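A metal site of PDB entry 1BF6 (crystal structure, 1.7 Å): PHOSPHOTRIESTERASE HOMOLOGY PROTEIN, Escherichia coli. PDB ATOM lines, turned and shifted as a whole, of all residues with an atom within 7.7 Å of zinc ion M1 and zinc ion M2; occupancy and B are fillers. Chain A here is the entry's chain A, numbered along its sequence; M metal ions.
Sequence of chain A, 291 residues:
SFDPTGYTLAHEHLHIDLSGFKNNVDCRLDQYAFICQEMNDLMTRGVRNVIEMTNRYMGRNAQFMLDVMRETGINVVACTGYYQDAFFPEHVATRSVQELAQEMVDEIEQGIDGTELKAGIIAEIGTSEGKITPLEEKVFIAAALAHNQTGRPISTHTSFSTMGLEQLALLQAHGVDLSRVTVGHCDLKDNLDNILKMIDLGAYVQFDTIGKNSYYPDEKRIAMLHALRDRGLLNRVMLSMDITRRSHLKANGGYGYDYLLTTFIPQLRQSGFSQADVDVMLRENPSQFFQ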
ATOM      1  N   HIS A  11     -33.965  24.497  -4.683  1.00  0.00           N
ATOM      2  CA  HIS A  11     -33.321  24.325  -5.999  1.00  0.00           C
ATOM      3  C   HIS A  11     -34.023  23.281  -6.842  1.00  0.00           C
ATOM      4  O   HIS A  11     -33.767  22.092  -6.704  1.00  0.00           O
ATOM      5  CB  HIS A  11     -31.872  23.898  -5.798  1.00  0.00           C
ATOM      6  CG  HIS A  11     -31.063  23.879  -7.062  1.00  0.00           C
ATOM      7  ND1 HIS A  11     -29.971  24.706  -7.277  1.00  0.00           N
ATOM      8  CD2 HIS A  11     -31.216  23.147  -8.186  1.00  0.00           C
ATOM      9  CE1 HIS A  11     -29.500  24.453  -8.499  1.00  0.00           C
ATOM     10  NE2 HIS A  11     -30.213  23.519  -9.092  1.00  0.00           N
ATOM     11  N   GLU A  12     -34.867  23.743  -7.749  1.00  0.00           N
ATOM     12  CA  GLU A  12     -35.628  22.861  -8.611  1.00  0.00           C
ATOM     13  C   GLU A  12     -35.757  23.395 -10.031  1.00  0.00           C
ATOM     14  O   GLU A  12     -35.441  24.559 -10.318  1.00  0.00           O
ATOM     15  CB  GLU A  12     -37.050  22.685  -8.069  1.00  0.00           C
ATOM     16  CG  GLU A  12     -37.142  22.077  -6.679  1.00  0.00           C
ATOM     17  CD  GLU A  12     -36.529  20.707  -6.599  1.00  0.00           C
ATOM     18  OE1 GLU A  12     -36.460  19.993  -7.623  1.00  0.00           O
ATOM     19  OE2 GLU A  12     -36.089  20.333  -5.492  1.00  0.00           O
ATOM     20  N   HIS A  13     -36.230  22.532 -10.923  1.00  0.00           N
ATOM     21  CA  HIS A  13     -36.501  22.899 -12.290  1.00  0.00           C
ATOM     22  C   HIS A  13     -37.911  22.431 -12.578  1.00  0.00           C
ATOM     23  O   HIS A  13     -38.226  21.276 -12.271  1.00  0.00           O
ATOM     24  CB  HIS A  13     -35.535  22.210 -13.251  1.00  0.00           C
ATOM     25  CG  HIS A  13     -34.126  22.650 -13.077  1.00  0.00           C
ATOM     26  ND1 HIS A  13     -33.616  23.815 -13.604  1.00  0.00           N
ATOM     27  CD2 HIS A  13     -33.130  22.108 -12.343  1.00  0.00           C
ATOM     28  CE1 HIS A  13     -32.368  23.946 -13.170  1.00  0.00           C
ATOM     29  NE2 HIS A  13     -32.035  22.930 -12.404  1.00  0.00           N
ATOM     30  N   ILE A  16     -37.210  22.985 -17.888  1.00  0.00           N
ATOM     31  CA  ILE A  16     -35.831  23.084 -18.325  1.00  0.00           C
ATOM     32  C   ILE A  16     -35.702  22.254 -19.583  1.00  0.00           C
ATOM     33  O   ILE A  16     -36.395  21.237 -19.737  1.00  0.00           O
ATOM     34  CB  ILE A  16     -34.833  22.608 -17.234  1.00  0.00           C
ATOM     35  CG1 ILE A  16     -33.398  22.730 -17.741  1.00  0.00           C
ATOM     36  CG2 ILE A  16     -35.151  21.168 -16.793  1.00  0.00           C
ATOM     37  CD1 ILE A  16     -32.338  22.468 -16.699  1.00  0.00           C
ATOM     38  N   GLU A  52     -37.061  28.140  -8.700  1.00  0.00           N
ATOM     39  CA  GLU A  52     -36.743  27.589 -10.004  1.00  0.00           C
ATOM     40  C   GLU A  52     -35.382  28.098 -10.518  1.00  0.00           C
ATOM     41  O   GLU A  52     -35.171  29.308 -10.676  1.00  0.00           O
ATOM     42  CB  GLU A  52     -37.895  27.898 -10.953  1.00  0.00           C
ATOM     43  CG  GLU A  52     -38.260  26.736 -11.873  1.00  0.00           C
ATOM     44  CD  GLU A  52     -37.408  26.688 -13.121  1.00  0.00           C
ATOM     45  OE1 GLU A  52     -36.695  27.665 -13.400  1.00  0.00           O
ATOM     46  OE2 GLU A  52     -37.463  25.661 -13.849  1.00  0.00           O
ATOM     47  N   MET A  53     -34.487  27.148 -10.815  1.00  0.00           N
ATOM     48  CA  MET A  53     -33.114  27.402 -11.224  1.00  0.00           C
ATOM     49  C   MET A  53     -32.771  27.420 -12.716  1.00  0.00           C
ATOM     50  O   MET A  53     -31.588  27.407 -13.075  1.00  0.00           O
ATOM     51  CB  MET A  53     -32.214  26.358 -10.566  1.00  0.00           C
ATOM     52  CG  MET A  53     -32.308  26.323  -9.042  1.00  0.00           C
ATOM     53  SD  MET A  53     -31.394  27.683  -8.247  1.00  0.00           S
ATOM     54  CE  MET A  53     -32.695  28.707  -7.862  1.00  0.00           C
ATOM     55  N   THR A  54     -33.788  27.432 -13.574  1.00  0.00           N
ATOM     56  CA  THR A  54     -33.578  27.415 -15.013  1.00  0.00           C
ATOM     57  C   THR A  54     -33.428  28.842 -15.557  1.00  0.00           C
ATOM     58  O   THR A  54     -34.406  29.562 -15.616  1.00  0.00           O
ATOM     59  CB  THR A  54     -34.780  26.759 -15.771  1.00  0.00           C
ATOM     60  OG1 THR A  54     -35.097  25.486 -15.185  1.00  0.00           O
ATOM     61  CG2 THR A  54     -34.456  26.548 -17.248  1.00  0.00           C
ATOM     62  N   MET A  58     -30.998  27.847 -20.539  1.00  0.00           N
ATOM     63  CA  MET A  58     -31.103  26.497 -20.015  1.00  0.00           C
ATOM     64  C   MET A  58     -32.485  25.998 -20.443  1.00  0.00           C
ATOM     65  O   MET A  58     -32.861  24.853 -20.188  1.00  0.00           O
ATOM     66  CB  MET A  58     -30.999  26.491 -18.479  1.00  0.00           C
ATOM     67  CG  MET A  58     -29.585  26.590 -17.936  1.00  0.00           C
ATOM     68  SD  MET A  58     -29.545  26.905 -16.160  1.00  0.00           S
ATOM     69  CE  MET A  58     -29.786  25.207 -15.511  1.00  0.00           C
ATOM     70  N   TYR A  83     -25.489  29.604 -17.003  1.00  0.00           N
ATOM     71  CA  TYR A  83     -25.161  28.293 -16.424  1.00  0.00           C
ATOM     72  C   TYR A  83     -23.705  27.938 -16.138  1.00  0.00           C
ATOM     73  O   TYR A  83     -23.234  28.124 -15.020  1.00  0.00           O
ATOM     74  CB  TYR A  83     -25.864  27.235 -17.271  1.00  0.00           C
ATOM     75  CG  TYR A  83     -25.946  25.857 -16.647  1.00  0.00           C
ATOM     76  CD1 TYR A  83     -25.914  25.670 -15.268  1.00  0.00           C
ATOM     77  CD2 TYR A  83     -26.056  24.724 -17.459  1.00  0.00           C
ATOM     78  CE1 TYR A  83     -25.984  24.403 -14.710  1.00  0.00           C
ATOM     79  CE2 TYR A  83     -26.122  23.456 -16.924  1.00  0.00           C
ATOM     80  CZ  TYR A  83     -26.088  23.301 -15.555  1.00  0.00           C
ATOM     81  OH  TYR A  83     -26.114  22.023 -15.046  1.00  0.00           O
ATOM     82  N   GLN A  84     -23.031  27.290 -17.077  1.00  0.00           N
ATOM     83  CA  GLN A  84     -21.628  26.920 -16.915  1.00  0.00           C
ATOM     84  C   GLN A  84     -20.968  26.915 -18.281  1.00  0.00           C
ATOM     85  O   GLN A  84     -21.653  26.968 -19.311  1.00  0.00           O
ATOM     86  CB  GLN A  84     -21.438  25.575 -16.204  1.00  0.00           C
ATOM     87  CG  GLN A  84     -22.209  24.434 -16.806  1.00  0.00           C
ATOM     88  CD  GLN A  84     -21.853  23.125 -16.160  1.00  0.00           C
ATOM     89  OE1 GLN A  84     -20.696  22.729 -16.119  1.00  0.00           O
ATOM     90  NE2 GLN A  84     -22.865  22.431 -15.639  1.00  0.00           N
ATOM     91  N   GLU A 124     -29.186  29.586 -11.783  1.00  0.00           N
ATOM     92  CA  GLU A 124     -28.149  28.894 -11.159  1.00  0.00           C
ATOM     93  C   GLU A 124     -26.803  29.227 -11.804  1.00  0.00           C
ATOM     94  O   GLU A 124     -26.730  28.959 -13.015  1.00  0.00           O
ATOM     95  CB  GLU A 124     -28.209  27.380 -10.828  1.00  0.00           C
ATOM     96  CG  GLU A 124     -28.391  26.503 -12.087  1.00  0.00           C
ATOM     97  CD  GLU A 124     -28.421  25.019 -11.574  1.00  0.00           C
ATOM     98  OE1 GLU A 124     -27.344  24.902 -11.054  1.00  0.00           O
ATOM     99  OE2 GLU A 124     -29.493  24.645 -11.991  1.00  0.00           O
ATOM    100  N   ILE A 125     -25.934  29.980 -11.142  1.00  0.00           N
ATOM    101  CA  ILE A 125     -24.681  30.336 -11.771  1.00  0.00           C
ATOM    102  C   ILE A 125     -23.629  29.336 -11.367  1.00  0.00           C
ATOM    103  O   ILE A 125     -23.312  29.164 -10.192  1.00  0.00           O
ATOM    104  CB  ILE A 125     -24.302  31.832 -11.532  1.00  0.00           C
ATOM    105  CG1 ILE A 125     -24.069  32.121 -10.058  1.00  0.00           C
ATOM    106  CG2 ILE A 125     -25.470  32.737 -12.018  1.00  0.00           C
ATOM    107  CD1 ILE A 125     -23.528  33.540  -9.812  1.00  0.00           C
ATOM    108  N   GLY A 126     -23.136  28.604 -12.362  1.00  0.00           N
ATOM    109  CA  GLY A 126     -22.164  27.572 -12.070  1.00  0.00           C
ATOM    110  C   GLY A 126     -20.740  27.660 -12.557  1.00  0.00           C
ATOM    111  O   GLY A 126     -20.344  28.535 -13.343  1.00  0.00           O
ATOM    112  N   THR A 156     -25.802  29.393  -6.532  1.00  0.00           N
ATOM    113  CA  THR A 156     -24.854  28.755  -7.433  1.00  0.00           C
ATOM    114  C   THR A 156     -24.990  27.253  -7.733  1.00  0.00           C
ATOM    115  O   THR A 156     -25.779  26.540  -7.110  1.00  0.00           O
ATOM    116  CB  THR A 156     -23.411  28.990  -6.936  1.00  0.00           C
ATOM    117  OG1 THR A 156     -23.093  28.024  -5.919  1.00  0.00           O
ATOM    118  CG2 THR A 156     -23.240  30.415  -6.357  1.00  0.00           C
ATOM    119  N   HIS A 157     -24.182  26.792  -8.691  1.00  0.00           N
ATOM    120  CA  HIS A 157     -24.079  25.386  -9.104  1.00  0.00           C
ATOM    121  C   HIS A 157     -22.620  24.997  -8.940  1.00  0.00           C
ATOM    122  O   HIS A 157     -21.742  25.632  -9.540  1.00  0.00           O
ATOM    123  CB  HIS A 157     -24.454  25.184 -10.595  1.00  0.00           C
ATOM    124  CG  HIS A 157     -23.945  23.901 -11.204  1.00  0.00           C
ATOM    125  ND1 HIS A 157     -24.804  22.884 -11.566  1.00  0.00           N
ATOM    126  CD2 HIS A 157     -22.687  23.560 -11.588  1.00  0.00           C
ATOM    127  CE1 HIS A 157     -24.060  21.961 -12.152  1.00  0.00           C
ATOM    128  NE2 HIS A 157     -22.768  22.333 -12.191  1.00  0.00           N
ATOM    129  N   THR A 158     -22.330  24.024  -8.081  1.00  0.00           N
ATOM    130  CA  THR A 158     -20.966  23.539  -7.974  1.00  0.00           C
ATOM    131  C   THR A 158     -21.030  22.179  -8.684  1.00  0.00           C
ATOM    132  O   THR A 158     -22.010  21.434  -8.528  1.00  0.00           O
ATOM    133  CB  THR A 158     -20.428  23.346  -6.520  1.00  0.00           C
ATOM    134  OG1 THR A 158     -21.244  22.410  -5.795  1.00  0.00           O
ATOM    135  CG2 THR A 158     -20.341  24.682  -5.780  1.00  0.00           C
ATOM    136  N   SER A 159     -20.050  21.924  -9.547  1.00  0.00           N
ATOM    137  CA  SER A 159     -19.980  20.673 -10.284  1.00  0.00           C
ATOM    138  C   SER A 159     -19.366  19.605  -9.388  1.00  0.00           C
ATOM    139  O   SER A 159     -18.194  19.671  -9.027  1.00  0.00           O
ATOM    140  CB  SER A 159     -19.179  20.858 -11.573  1.00  0.00           C
ATOM    141  OG  SER A 159     -19.970  21.509 -12.542  1.00  0.00           O
ATOM    142  N   GLY A 184     -24.927  25.835  -4.224  1.00  0.00           N
ATOM    143  CA  GLY A 184     -25.645  24.644  -4.653  1.00  0.00           C
ATOM    144  C   GLY A 184     -24.810  23.379  -4.797  1.00  0.00           C
ATOM    145  O   GLY A 184     -23.602  23.443  -5.038  1.00  0.00           O
ATOM    146  N   HIS A 185     -25.472  22.231  -4.633  1.00  0.00           N
ATOM    147  CA  HIS A 185     -24.846  20.912  -4.748  1.00  0.00           C
ATOM    148  C   HIS A 185     -23.646  20.641  -3.871  1.00  0.00           C
ATOM    149  O   HIS A 185     -22.617  20.165  -4.350  1.00  0.00           O
ATOM    150  CB  HIS A 185     -24.457  20.637  -6.198  1.00  0.00           C
ATOM    151  CG  HIS A 185     -25.442  21.125  -7.196  1.00  0.00           C
ATOM    152  ND1 HIS A 185     -26.813  21.073  -7.021  1.00  0.00           N
ATOM    153  CD2 HIS A 185     -25.243  21.757  -8.374  1.00  0.00           C
ATOM    154  CE1 HIS A 185     -27.370  21.670  -8.059  1.00  0.00           C
ATOM    155  NE2 HIS A 185     -26.438  22.083  -8.883  1.00  0.00           N
ATOM    156  N   ASP A 208     -29.028  19.740  -2.103  1.00  0.00           N
ATOM    157  CA  ASP A 208     -30.100  19.752  -3.111  1.00  0.00           C
ATOM    158  C   ASP A 208     -30.097  18.640  -4.165  1.00  0.00           C
ATOM    159  O   ASP A 208     -30.769  18.764  -5.188  1.00  0.00           O
ATOM    160  CB  ASP A 208     -30.125  21.106  -3.839  1.00  0.00           C
ATOM    161  CG  ASP A 208     -28.762  21.518  -4.373  1.00  0.00           C
ATOM    162  OD1 ASP A 208     -27.928  20.630  -4.667  1.00  0.00           O
ATOM    163  OD2 ASP A 208     -28.505  22.740  -4.449  1.00  0.00           O
ATOM    164  N   THR A 209     -29.309  17.586  -3.937  1.00  0.00           N
ATOM    165  CA  THR A 209     -29.263  16.459  -4.862  1.00  0.00           C
ATOM    166  C   THR A 209     -29.829  15.207  -4.162  1.00  0.00           C
ATOM    167  O   THR A 209     -29.460  14.062  -4.488  1.00  0.00           O
ATOM    168  CB  THR A 209     -27.840  16.201  -5.399  1.00  0.00           C
ATOM    169  OG1 THR A 209     -26.935  15.937  -4.313  1.00  0.00           O
ATOM    170  CG2 THR A 209     -27.325  17.411  -6.201  1.00  0.00           C
ATOM    171  N   LYS A 212     -30.444  11.427  -5.545  1.00  0.00           N
ATOM    172  CA  LYS A 212     -29.505  11.077  -6.614  1.00  0.00           C
ATOM    173  C   LYS A 212     -28.412  10.182  -6.038  1.00  0.00           C
ATOM    174  O   LYS A 212     -27.226  10.498  -6.034  1.00  0.00           O
ATOM    175  CB  LYS A 212     -28.926  12.363  -7.251  1.00  0.00           C
ATOM    176  CG  LYS A 212     -30.044  13.264  -7.791  1.00  0.00           C
ATOM    177  CD  LYS A 212     -29.596  14.374  -8.728  1.00  0.00           C
ATOM    178  CE  LYS A 212     -30.825  15.068  -9.290  1.00  0.00           C
ATOM    179  NZ  LYS A 212     -30.487  16.048 -10.348  1.00  0.00           N
ATOM    180  N   MET A 241     -34.258  18.666  -4.303  1.00  0.00           N
ATOM    181  CA  MET A 241     -34.075  17.450  -5.118  1.00  0.00           C
ATOM    182  C   MET A 241     -33.342  17.721  -6.439  1.00  0.00           C
ATOM    183  O   MET A 241     -32.757  16.807  -7.044  1.00  0.00           O
ATOM    184  CB  MET A 241     -35.451  16.862  -5.461  1.00  0.00           C
ATOM    185  CG  MET A 241     -36.378  16.560  -4.284  1.00  0.00           C
ATOM    186  SD  MET A 241     -35.694  15.305  -3.252  1.00  0.00           S
ATOM    187  CE  MET A 241     -35.815  13.906  -4.355  1.00  0.00           C
ATOM    188  N   ASP A 242     -33.408  18.963  -6.899  1.00  0.00           N
ATOM    189  CA  ASP A 242     -32.830  19.366  -8.183  1.00  0.00           C
ATOM    190  C   ASP A 242     -33.346  18.453  -9.316  1.00  0.00           C
ATOM    191  O   ASP A 242     -32.549  17.844 -10.044  1.00  0.00           O
ATOM    192  CB  ASP A 242     -31.291  19.330  -8.150  1.00  0.00           C
ATOM    193  CG  ASP A 242     -30.661  19.913  -9.409  1.00  0.00           C
ATOM    194  OD1 ASP A 242     -31.358  20.657 -10.142  1.00  0.00           O
ATOM    195  OD2 ASP A 242     -29.487  19.622  -9.656  1.00  0.00           O
ATOM    196  N   ILE A 243     -34.679  18.326  -9.416  1.00  0.00           N
ATOM    197  CA  ILE A 243     -35.306  17.525 -10.474  1.00  0.00           C
ATOM    198  C   ILE A 243     -34.949  18.191 -11.813  1.00  0.00           C
ATOM    199  O   ILE A 243     -35.076  19.412 -11.964  1.00  0.00           O
ATOM    200  CB  ILE A 243     -36.857  17.472 -10.309  1.00  0.00           C
ATOM    201  CG1 ILE A 243     -37.235  16.733  -9.021  1.00  0.00           C
ATOM    202  CG2 ILE A 243     -37.503  16.823 -11.519  1.00  0.00           C
ATOM    203  CD1 ILE A 243     -36.690  15.320  -8.929  1.00  0.00           C
ATOM    204  N   THR A 244     -34.494  17.376 -12.765  1.00  0.00           N
ATOM    205  CA  THR A 244     -34.066  17.868 -14.071  1.00  0.00           C
ATOM    206  C   THR A 244     -34.524  17.023 -15.280  1.00  0.00           C
ATOM    207  O   THR A 244     -34.447  17.483 -16.417  1.00  0.00           O
ATOM    208  CB  THR A 244     -32.520  17.922 -14.158  1.00  0.00           C
ATOM    209  OG1 THR A 244     -31.973  16.614 -13.943  1.00  0.00           O
ATOM    210  CG2 THR A 244     -31.915  18.876 -13.119  1.00  0.00           C
HETATM  211 ZN    ZN M   1     -30.303  22.574 -11.162  1.00  0.00          ZN
HETATM  212 ZN    ZN M   2     -26.972  22.753 -10.887  1.00  0.00          ZN
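Within 4 Å of zinc ion M1: His 11, His 13, Glu 124 and Asp 242.
The nearest printed residue that does not touch zinc ion M1 is Met 53 (4.3 Å).
Of the 26 residues printed, 4 come within 4 Å of zinc ion M2.
Zinc ion M1 is bound by NE2 of His 13, NE2 of His 11, OE2 of Glu 124 and OD1 of Asp 242.
The backbone carbonyl oxygen (O) of Ile 125 lies within hydrogen-bond range of the backbone NH (N) of His 157, at 2.9 Å.
The side-chain sulfur (SD) of Met 53 lies close to a ring nitrogen (ND1) of His 11 (3.4 Å).
N of Glu 124 lies close to O of Met 53, at 3.5 Å.
The backbone NH of Asp 242 lies close to the backbone carbonyl oxygen of Asp 208.
ND1 of His 13 is in hydrogen-bond range of OG1 of Thr 54, 2.7 Å away.
A ring nitrogen (ND1) of His 185 lies within hydrogen-bond range of the side-chain carboxylate of Asp 208, at 2.6 Å.
The backbone carbonyl oxygen of His 185 is in hydrogen-bond range of the side-chain hydroxyl of Thr 158, 3.0 Å away.
The side-chain carboxylate (OD2) of Asp 242 is in salt-bridge range of the side-chain amino group (NZ) of Lys 212, at 3.8 Å.
Zinc ion M2 is bound by NE2 of His 185 (2.2 Å), OE1 of Glu 124 (2.2 Å) and ND1 of His 157 (2.3 Å).
Zinc ion M2 has three donor atoms within binding distance.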
